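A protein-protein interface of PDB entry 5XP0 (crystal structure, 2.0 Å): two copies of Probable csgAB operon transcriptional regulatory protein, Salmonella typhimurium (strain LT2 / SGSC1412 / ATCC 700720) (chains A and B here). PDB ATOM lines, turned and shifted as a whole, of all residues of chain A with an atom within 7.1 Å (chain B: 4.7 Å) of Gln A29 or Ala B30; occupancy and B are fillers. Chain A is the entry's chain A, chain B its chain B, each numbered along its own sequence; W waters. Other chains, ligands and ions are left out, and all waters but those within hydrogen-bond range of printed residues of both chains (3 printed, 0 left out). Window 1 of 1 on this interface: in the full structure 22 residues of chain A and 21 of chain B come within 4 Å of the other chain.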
ATOM      1  N   LEU A  22      11.933   2.758  25.177  1.00  0.00           N
ATOM      2  CA  LEU A  22      11.853   4.050  24.534  1.00  0.00           C
ATOM      3  C   LEU A  22      10.388   4.452  24.575  1.00  0.00           C
ATOM      4  O   LEU A  22       9.540   3.756  24.009  1.00  0.00           O
ATOM      5  CB  LEU A  22      12.418   3.980  23.112  1.00  0.00           C
ATOM      6  CG  LEU A  22      12.073   5.168  22.214  1.00  0.00           C
ATOM      7  CD1 LEU A  22      12.776   6.356  22.796  1.00  0.00           C
ATOM      8  CD2 LEU A  22      12.524   4.877  20.789  1.00  0.00           C
ATOM      9  N   LYS A  25       6.292   8.673  20.632  1.00  0.00           N
ATOM     10  CA  LYS A  25       5.239   8.424  19.668  1.00  0.00           C
ATOM     11  C   LYS A  25       5.715   7.356  18.681  1.00  0.00           C
ATOM     12  O   LYS A  25       6.766   7.513  18.070  1.00  0.00           O
ATOM     13  CB  LYS A  25       4.850   9.708  18.939  1.00  0.00           C
ATOM     14  CG  LYS A  25       3.835   9.486  17.808  1.00  0.00           C
ATOM     15  CD  LYS A  25       3.239  10.780  17.251  1.00  0.00           C
ATOM     16  CE  LYS A  25       4.260  11.801  16.872  1.00  0.00           C
ATOM     17  NZ  LYS A  25       3.554  13.027  16.440  1.00  0.00           N
ATOM     18  N   PRO A  26       4.979   6.278  18.488  1.00  0.00           N
ATOM     19  CA  PRO A  26       5.468   5.228  17.585  1.00  0.00           C
ATOM     20  C   PRO A  26       5.577   5.765  16.165  1.00  0.00           C
ATOM     21  O   PRO A  26       4.724   6.509  15.695  1.00  0.00           O
ATOM     22  CB  PRO A  26       4.403   4.119  17.691  1.00  0.00           C
ATOM     23  CG  PRO A  26       3.673   4.412  18.977  1.00  0.00           C
ATOM     24  CD  PRO A  26       3.716   5.911  19.152  1.00  0.00           C
ATOM     25  N   SER A  27       6.653   5.414  15.495  1.00  0.00           N
ATOM     26  CA  SER A  27       6.915   5.958  14.175  1.00  0.00           C
ATOM     27  C   SER A  27       8.059   5.139  13.620  1.00  0.00           C
ATOM     28  O   SER A  27       8.766   4.455  14.373  1.00  0.00           O
ATOM     29  CB  SER A  27       7.297   7.448  14.254  1.00  0.00           C
ATOM     30  OG  SER A  27       8.575   7.491  14.870  1.00  0.00           O
ATOM     31  N   LEU A  28       8.214   5.174  12.293  1.00  0.00           N
ATOM     32  CA  LEU A  28       9.326   4.454  11.700  1.00  0.00           C
ATOM     33  C   LEU A  28      10.628   4.964  12.278  1.00  0.00           C
ATOM     34  O   LEU A  28      11.556   4.188  12.554  1.00  0.00           O
ATOM     35  CB  LEU A  28       9.311   4.592  10.160  1.00  0.00           C
ATOM     36  CG  LEU A  28      10.436   3.818   9.438  1.00  0.00           C
ATOM     37  CD1 LEU A  28      10.228   2.343   9.558  1.00  0.00           C
ATOM     38  CD2 LEU A  28      10.514   4.203   7.963  1.00  0.00           C
ATOM     39  N   GLN A  29      10.725   6.277  12.475  1.00  0.00           N
ATOM     40  CA  GLN A  29      11.987   6.795  12.949  1.00  0.00           C
ATOM     41  C   GLN A  29      12.245   6.347  14.379  1.00  0.00           C
ATOM     42  O   GLN A  29      13.383   6.026  14.714  1.00  0.00           O
ATOM     43  CB  GLN A  29      12.069   8.315  12.771  1.00  0.00           C
ATOM     44  CG  GLN A  29      11.054   9.177  13.447  1.00  0.00           C
ATOM     45  CD  GLN A  29       9.861   9.450  12.520  1.00  0.00           C
ATOM     46  OE1 GLN A  29       9.352   8.537  11.842  1.00  0.00           O
ATOM     47  NE2 GLN A  29       9.432  10.691  12.474  1.00  0.00           N
ATOM     48  N   ALA A  30      11.207   6.223  15.212  1.00  0.00           N
ATOM     49  CA  ALA A  30      11.430   5.704  16.562  1.00  0.00           C
ATOM     50  C   ALA A  30      11.961   4.275  16.528  1.00  0.00           C
ATOM     51  O   ALA A  30      12.901   3.930  17.260  1.00  0.00           O
ATOM     52  CB  ALA A  30      10.127   5.774  17.362  1.00  0.00           C
ATOM     53  N   THR A  31      11.402   3.433  15.662  1.00  0.00           N
ATOM     54  CA  THR A  31      11.947   2.095  15.515  1.00  0.00           C
ATOM     55  C   THR A  31      13.382   2.152  15.034  1.00  0.00           C
ATOM     56  O   THR A  31      14.218   1.375  15.507  1.00  0.00           O
ATOM     57  CB  THR A  31      11.119   1.221  14.562  1.00  0.00           C
ATOM     58  OG1 THR A  31      11.141   1.789  13.251  1.00  0.00           O
ATOM     59  CG2 THR A  31       9.778   1.180  15.007  1.00  0.00           C
ATOM     60  N   ALA A  32      13.709   3.084  14.113  1.00  0.00           N
ATOM     61  CA  ALA A  32      15.077   3.190  13.629  1.00  0.00           C
ATOM     62  C   ALA A  32      16.037   3.544  14.764  1.00  0.00           C
ATOM     63  O   ALA A  32      17.144   3.006  14.844  1.00  0.00           O
ATOM     64  CB  ALA A  32      15.198   4.225  12.510  1.00  0.00           C
ATOM     65  N   LEU A  33      15.654   4.465  15.625  1.00  0.00           N
ATOM     66  CA  LEU A  33      16.539   4.822  16.743  1.00  0.00           C
ATOM     67  C   LEU A  33      16.676   3.652  17.716  1.00  0.00           C
ATOM     68  O   LEU A  33      17.790   3.305  18.140  1.00  0.00           O
ATOM     69  CB  LEU A  33      15.999   6.069  17.474  1.00  0.00           C
ATOM     70  CG  LEU A  33      16.755   6.477  18.738  1.00  0.00           C
ATOM     71  CD1 LEU A  33      18.139   6.928  18.387  1.00  0.00           C
ATOM     72  CD2 LEU A  33      16.018   7.547  19.598  1.00  0.00           C
ATOM     73  N   LEU A  34      15.555   3.005  18.050  1.00  0.00           N
ATOM     74  CA  LEU A  34      15.617   1.884  18.987  1.00  0.00           C
ATOM     75  C   LEU A  34      16.558   0.814  18.473  1.00  0.00           C
ATOM     76  O   LEU A  34      17.410   0.325  19.215  1.00  0.00           O
ATOM     77  CB  LEU A  34      14.220   1.313  19.243  1.00  0.00           C
ATOM     78  CG  LEU A  34      14.138   0.162  20.257  1.00  0.00           C
ATOM     79  CD1 LEU A  34      14.587   0.644  21.655  1.00  0.00           C
ATOM     80  CD2 LEU A  34      12.754  -0.390  20.328  1.00  0.00           C
ATOM     81  N   GLN A  35      16.449   0.465  17.189  1.00  0.00           N
ATOM     82  CA  GLN A  35      17.330  -0.541  16.624  1.00  0.00           C
ATOM     83  C   GLN A  35      18.784  -0.097  16.708  1.00  0.00           C
ATOM     84  O   GLN A  35      19.671  -0.914  17.008  1.00  0.00           O
ATOM     85  CB  GLN A  35      16.959  -0.827  15.167  1.00  0.00           C
ATOM     86  CG  GLN A  35      15.634  -1.559  15.047  1.00  0.00           C
ATOM     87  CD  GLN A  35      15.735  -3.001  15.549  1.00  0.00           C
ATOM     88  OE1 GLN A  35      15.117  -3.370  16.549  1.00  0.00           O
ATOM     89  NE2 GLN A  35      16.536  -3.817  14.858  1.00  0.00           N
ATOM     90  N   LEU A  47       9.706  -0.377  22.338  1.00  0.00           N
ATOM     91  CA  LEU A  47       9.097   0.915  22.142  1.00  0.00           C
ATOM     92  C   LEU A  47       7.772   0.891  22.884  1.00  0.00           C
ATOM     93  O   LEU A  47       7.020  -0.077  22.778  1.00  0.00           O
ATOM     94  CB  LEU A  47       8.895   1.127  20.642  1.00  0.00           C
ATOM     95  CG  LEU A  47       8.759   2.533  20.063  1.00  0.00           C
ATOM     96  CD1 LEU A  47       8.740   2.426  18.512  1.00  0.00           C
ATOM     97  CD2 LEU A  47       7.522   3.188  20.593  1.00  0.00           C
ATOM     98  N   ASN A  95      15.451  14.205  23.748  1.00  0.00           N
ATOM     99  CA  ASN A  95      14.973  15.363  23.000  1.00  0.00           C
ATOM    100  C   ASN A  95      14.570  16.504  23.934  1.00  0.00           C
ATOM    101  O   ASN A  95      13.593  17.203  23.692  1.00  0.00           O
ATOM    102  CB  ASN A  95      13.790  15.007  22.069  1.00  0.00           C
ATOM    103  CG  ASN A  95      14.155  13.928  21.025  1.00  0.00           C
ATOM    104  OD1 ASN A  95      15.236  13.964  20.430  1.00  0.00           O
ATOM    105  ND2 ASN A  95      13.244  12.954  20.804  1.00  0.00           N
ATOM    106  N   THR A 118      19.495  16.571  19.224  1.00  0.00           N
ATOM    107  CA  THR A 118      18.624  15.875  18.284  1.00  0.00           C
ATOM    108  C   THR A 118      19.365  15.491  17.000  1.00  0.00           C
ATOM    109  O   THR A 118      18.749  14.945  16.086  1.00  0.00           O
ATOM    110  CB  THR A 118      17.400  16.742  17.955  1.00  0.00           C
ATOM    111  OG1 THR A 118      17.827  18.021  17.469  1.00  0.00           O
ATOM    112  CG2 THR A 118      16.485  16.947  19.197  1.00  0.00           C
ATOM    113  N   LEU B  22      13.931  14.798   4.443  1.00  0.00           N
ATOM    114  CA  LEU B  22      13.017  14.211   5.391  1.00  0.00           C
ATOM    115  C   LEU B  22      12.316  15.351   6.117  1.00  0.00           C
ATOM    116  O   LEU B  22      12.936  16.104   6.873  1.00  0.00           O
ATOM    117  CB  LEU B  22      13.779  13.281   6.324  1.00  0.00           C
ATOM    118  CG  LEU B  22      12.998  12.847   7.571  1.00  0.00           C
ATOM    119  CD1 LEU B  22      11.804  12.049   7.194  1.00  0.00           C
ATOM    120  CD2 LEU B  22      13.889  11.978   8.361  1.00  0.00           C
ATOM    121  N   THR B  24       9.748  16.344   8.792  1.00  0.00           N
ATOM    122  CA  THR B  24       9.152  15.727   9.963  1.00  0.00           C
ATOM    123  C   THR B  24       9.382  16.637  11.165  1.00  0.00           C
ATOM    124  O   THR B  24       9.831  17.783  11.033  1.00  0.00           O
ATOM    125  CB  THR B  24       9.769  14.350  10.177  1.00  0.00           C
ATOM    126  OG1 THR B  24       9.135  13.707  11.303  1.00  0.00           O
ATOM    127  CG2 THR B  24      11.231  14.527  10.404  1.00  0.00           C
ATOM    128  N   LYS B  25       9.099  16.114  12.346  1.00  0.00           N
ATOM    129  CA  LYS B  25       9.457  16.821  13.573  1.00  0.00           C
ATOM    130  C   LYS B  25      10.917  16.533  13.872  1.00  0.00           C
ATOM    131  O   LYS B  25      11.291  15.356  13.999  1.00  0.00           O
ATOM    132  CB  LYS B  25       8.621  16.326  14.740  1.00  0.00           C
ATOM    133  CG  LYS B  25       9.058  16.907  16.098  1.00  0.00           C
ATOM    134  CD  LYS B  25       8.209  16.344  17.233  1.00  0.00           C
ATOM    135  CE  LYS B  25       6.819  16.895  17.307  1.00  0.00           C
ATOM    136  NZ  LYS B  25       6.278  16.690  18.705  1.00  0.00           N
ATOM    137  N   SER B  27      14.089  15.535  15.639  1.00  0.00           N
ATOM    138  CA  SER B  27      14.200  14.699  16.819  1.00  0.00           C
ATOM    139  C   SER B  27      15.409  13.824  16.613  1.00  0.00           C
ATOM    140  O   SER B  27      15.820  13.563  15.471  1.00  0.00           O
ATOM    141  CB  SER B  27      12.962  13.819  17.017  1.00  0.00           C
ATOM    142  OG  SER B  27      12.900  12.839  15.987  1.00  0.00           O
ATOM    143  N   LEU B  28      15.945  13.316  17.726  1.00  0.00           N
ATOM    144  CA  LEU B  28      17.049  12.369  17.596  1.00  0.00           C
ATOM    145  C   LEU B  28      16.626  11.190  16.732  1.00  0.00           C
ATOM    146  O   LEU B  28      17.424  10.667  15.951  1.00  0.00           O
ATOM    147  CB  LEU B  28      17.508  11.865  18.957  1.00  0.00           C
ATOM    148  CG  LEU B  28      18.760  10.983  18.838  1.00  0.00           C
ATOM    149  CD1 LEU B  28      19.974  11.823  18.436  1.00  0.00           C
ATOM    150  CD2 LEU B  28      19.031  10.306  20.099  1.00  0.00           C
ATOM    151  N   GLN B  29      15.387  10.714  16.882  1.00  0.00           N
ATOM    152  CA  GLN B  29      15.028   9.544  16.103  1.00  0.00           C
ATOM    153  C   GLN B  29      14.895   9.853  14.611  1.00  0.00           C
ATOM    154  O   GLN B  29      15.242   9.005  13.793  1.00  0.00           O
ATOM    155  CB  GLN B  29      13.772   8.871  16.623  1.00  0.00           C
ATOM    156  CG  GLN B  29      12.607   9.705  16.700  1.00  0.00           C
ATOM    157  CD  GLN B  29      12.435  10.372  18.056  1.00  0.00           C
ATOM    158  OE1 GLN B  29      13.389  10.918  18.623  1.00  0.00           O
ATOM    159  NE2 GLN B  29      11.214  10.344  18.576  1.00  0.00           N
ATOM    160  N   ALA B  30      14.443  11.053  14.240  1.00  0.00           N
ATOM    161  CA  ALA B  30      14.441  11.432  12.824  1.00  0.00           C
ATOM    162  C   ALA B  30      15.850  11.445  12.251  1.00  0.00           C
ATOM    163  O   ALA B  30      16.084  11.002  11.120  1.00  0.00           O
ATOM    164  CB  ALA B  30      13.777  12.792  12.659  1.00  0.00           C
ATOM    165  N   THR B  31      16.806  11.951  13.010  1.00  0.00           N
ATOM    166  CA  THR B  31      18.191  11.907  12.578  1.00  0.00           C
ATOM    167  C   THR B  31      18.675  10.486  12.394  1.00  0.00           C
ATOM    168  O   THR B  31      19.384  10.187  11.416  1.00  0.00           O
ATOM    169  CB  THR B  31      19.072  12.643  13.613  1.00  0.00           C
ATOM    170  OG1 THR B  31      18.701  14.018  13.621  1.00  0.00           O
ATOM    171  CG2 THR B  31      20.562  12.482  13.301  1.00  0.00           C
ATOM    172  N   ALA B  32      18.319   9.595  13.319  1.00  0.00           N
ATOM    173  CA  ALA B  32      18.719   8.196  13.194  1.00  0.00           C
ATOM    174  C   ALA B  32      18.131   7.586  11.936  1.00  0.00           C
ATOM    175  O   ALA B  32      18.803   6.822  11.239  1.00  0.00           O
ATOM    176  CB  ALA B  32      18.274   7.356  14.394  1.00  0.00           C
ATOM    177  N   LEU B  33      16.869   7.879  11.642  1.00  0.00           N
ATOM    178  CA  LEU B  33      16.301   7.325  10.414  1.00  0.00           C
ATOM    179  C   LEU B  33      16.992   7.915   9.199  1.00  0.00           C
ATOM    180  O   LEU B  33      17.366   7.198   8.273  1.00  0.00           O
ATOM    181  CB  LEU B  33      14.801   7.591  10.320  1.00  0.00           C
ATOM    182  CG  LEU B  33      14.156   7.122   9.009  1.00  0.00           C
ATOM    183  CD1 LEU B  33      14.191   5.632   8.772  1.00  0.00           C
ATOM    184  CD2 LEU B  33      12.709   7.573   9.021  1.00  0.00           C
ATOM    185  N   LEU B  34      17.189   9.223   9.190  1.00  0.00           N
ATOM    186  CA  LEU B  34      17.845   9.826   8.030  1.00  0.00           C
ATOM    187  C   LEU B  34      19.248   9.242   7.809  1.00  0.00           C
ATOM    188  O   LEU B  34      19.664   8.961   6.681  1.00  0.00           O
ATOM    189  CB  LEU B  34      17.902  11.321   8.219  1.00  0.00           C
ATOM    190  CG  LEU B  34      18.564  12.030   7.029  1.00  0.00           C
ATOM    191  CD1 LEU B  34      17.753  11.903   5.749  1.00  0.00           C
ATOM    192  CD2 LEU B  34      18.801  13.464   7.408  1.00  0.00           C
ATOM    193  N   LEU B  47      17.291  16.898   7.007  1.00  0.00           N
ATOM    194  CA  LEU B  47      16.073  16.932   7.795  1.00  0.00           C
ATOM    195  C   LEU B  47      15.500  18.334   7.734  1.00  0.00           C
ATOM    196  O   LEU B  47      16.243  19.301   7.861  1.00  0.00           O
ATOM    197  CB  LEU B  47      16.430  16.571   9.229  1.00  0.00           C
ATOM    198  CG  LEU B  47      15.423  16.065  10.242  1.00  0.00           C
ATOM    199  CD1 LEU B  47      16.204  15.592  11.479  1.00  0.00           C
ATOM    200  CD2 LEU B  47      14.467  17.172  10.622  1.00  0.00           C
ATOM    201  N   ASP B  66       6.365  13.357   6.528  1.00  0.00           N
ATOM    202  CA  ASP B  66       5.896  12.576   7.688  1.00  0.00           C
ATOM    203  C   ASP B  66       4.418  12.853   7.990  1.00  0.00           C
ATOM    204  O   ASP B  66       4.076  13.810   8.679  1.00  0.00           O
ATOM    205  CB  ASP B  66       6.747  12.887   8.908  1.00  0.00           C
ATOM    206  CG  ASP B  66       6.471  11.921  10.082  1.00  0.00           C
ATOM    207  OD1 ASP B  66       5.488  11.153  10.015  1.00  0.00           O
ATOM    208  OD2 ASP B  66       7.271  11.903  11.037  1.00  0.00           O
ATOM    209  N   LEU B  94       5.372   9.267   4.422  1.00  0.00           N
ATOM    210  CA  LEU B  94       5.938   8.420   5.438  1.00  0.00           C
ATOM    211  C   LEU B  94       4.960   8.307   6.599  1.00  0.00           C
ATOM    212  O   LEU B  94       4.202   9.238   6.869  1.00  0.00           O
ATOM    213  CB  LEU B  94       7.265   9.029   5.906  1.00  0.00           C
ATOM    214  CG  LEU B  94       8.144   8.238   6.856  1.00  0.00           C
ATOM    215  CD1 LEU B  94       8.815   7.116   6.069  1.00  0.00           C
ATOM    216  CD2 LEU B  94       9.198   9.184   7.507  1.00  0.00           C
ATOM    217  N   ASN B  95       4.979   7.155   7.273  1.00  0.00           N
ATOM    218  CA  ASN B  95       4.127   6.919   8.448  1.00  0.00           C
ATOM    219  C   ASN B  95       2.670   7.209   8.127  1.00  0.00           C
ATOM    220  O   ASN B  95       1.961   7.837   8.915  1.00  0.00           O
ATOM    221  CB  ASN B  95       4.555   7.752   9.659  1.00  0.00           C
ATOM    222  CG  ASN B  95       5.956   7.445  10.138  1.00  0.00           C
ATOM    223  OD1 ASN B  95       6.377   6.282  10.250  1.00  0.00           O
ATOM    224  ND2 ASN B  95       6.703   8.511  10.420  1.00  0.00           N
HETATM  225  O   HOH W   1      10.577  12.707  14.474  1.00  0.00           O
HETATM  226  O   HOH W   2       6.316  11.044  13.739  1.00  0.00           O
HETATM  227  O   HOH W   3       8.773   9.134  17.083  1.00  0.00           O
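N of Leu A28 lies within hydrogen-bond range of OD1 of Asn B95, at 3.0 Å.
The side-chain amide nitrogen (NE2) of Gln A29 is in hydrogen-bond range of the side-chain hydroxyl (OG1) of Thr B24, at 3.2 Å.
NE2 of Gln A29 sits at hydrogen-bond distance from OD2 of Asp B66 (2.9 Å).
OE1 of Gln A29 sits at hydrogen-bond distance from ND2 of Asn B95.
N of Leu B28 sits at hydrogen-bond distance from OD1 of Asn A95 (2.9 Å).
The side-chain amide oxygen (OE1) of Gln B29 is in hydrogen-bond range of the side-chain amide nitrogen (ND2) of Asn A95 (3.0 Å).
The backbone carbonyl oxygen (O) of Thr A118 sits at hydrogen-bond distance from the side-chain hydroxyl (OG1) of Thr B31 (2.6 Å).
The backbone carbonyl oxygen (O) of Ser B27 sits close to the backbone carbonyl oxygen (O) of Thr A118.
The backbone NH (N) of Ala A30 sits at hydrogen-bond distance from the side-chain hydroxyl (OG) of Ser A27 (2.9 Å).
The side-chain hydroxyl (OG1) of Thr A31 sits at hydrogen-bond distance from the backbone carbonyl oxygen (O) of Leu A28 (2.5 Å).
OD2 of Asp B66 is in hydrogen-bond range of OG1 of Thr B24.
OG of Ser B27 sits close to OE1 of Gln B29, 3.3 Å away.
OG of Ser B27 sits at hydrogen-bond distance from N of Ala B30, 2.9 Å away.
ND2 of Asn B95 sits at hydrogen-bond distance from OD1 of Asp B66, at 2.9 Å.
C of Ser A27 touches OD1 of Asn B95, 3.9 Å away.
Leu A28 touches Leu B94 (CD2 to CD1, 3.9 Å).
CB of Gln A29 touches N of Ala B30, at 3.9 Å.
Leu B33 touches Gln A29.
CB of Gln B29 touches CA of Ala A30, at 3.9 Å.
Leu B33 touches Ala A32.
Leu A33 touches Leu B28 (CD1 to CD2, 3.9 Å).
Leu A33 touches Gln B29.
Leu A33 touches Ala B32 (CA to CB, 3.9 Å).
O of Thr A118 touches CA of Leu B28 (3.4 Å).
Of chain B, only Thr B24 (3.2 Å), Gln B29 (3.4 Å), Ala B30 (3.9 Å), Leu B33 (3.7 Å), Asp B66 (2.9 Å) and Asn B95 (3.0 Å) come within 4 Å of Gln A29.
Ala B30 touches just one residue of chain A: Gln A29 (3.9 Å).
Of the printed residues of chain A, Asn B95 touches Ser A27 (3.9 Å), Leu A28 (3.0 Å) and Gln A29 (3.0 Å).
Of the printed residues of chain A, Ala B32 touches Leu A33 (3.9 Å).
Of the printed residues of chain B, Leu A33 touches Leu B28 (3.9 Å), Gln B29 (3.7 Å) and Ala B32 (3.9 Å).
Printed residues of chain A within 4 Å of Asp B66: Gln A29 (2.9 Å).
Thr A31 touches none of the printed residues of chain B.
Leu B22 touches none of the printed residues of chain A.
The nearest residue of chain B that does not touch Gln A29 is Leu B94 (4.4 Å).
The nearest printed residue of chain A that does not touch Ser B27 is Gln A29 (4.8 Å).
Hydrophobic or aromatic side chains of chain A that line the printed part of chain B: Leu A28, Ala A32 and Leu A33.
Among the printed residues, no Asp or Glu carboxylate lies within 4 Å of a Lys or Arg side-chain nitrogen of the other chain.
Ser A27 touches Asn B95, and with the chains exchanged Asn A95 touches Ser B27.
Leu A28 touches Asn B95, and with the chains exchanged Asn A95 touches Leu B28.
Gln B29 touches its own counterpart, Gln A29.
Gln A29 touches Asn B95, and with the chains exchanged Asn A95 touches Gln B29.
Of the 20 pairs that touch across the chains among the printed residues, 13 have their exchanged pair printed and touching as well.
Water W3 lies within hydrogen-bond range of O of Lys A25, OG of Ser A27 and NE2 of Gln B29.
Water W1 lies within hydrogen-bond range of OG of Ser B27, O of Lys B25 and NE2 of Gln A29.
Water W2 lies within hydrogen-bond range of the side-chain carboxylate (OD2) of Asp B66 and the side-chain amide nitrogen (NE2) of Gln A29.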
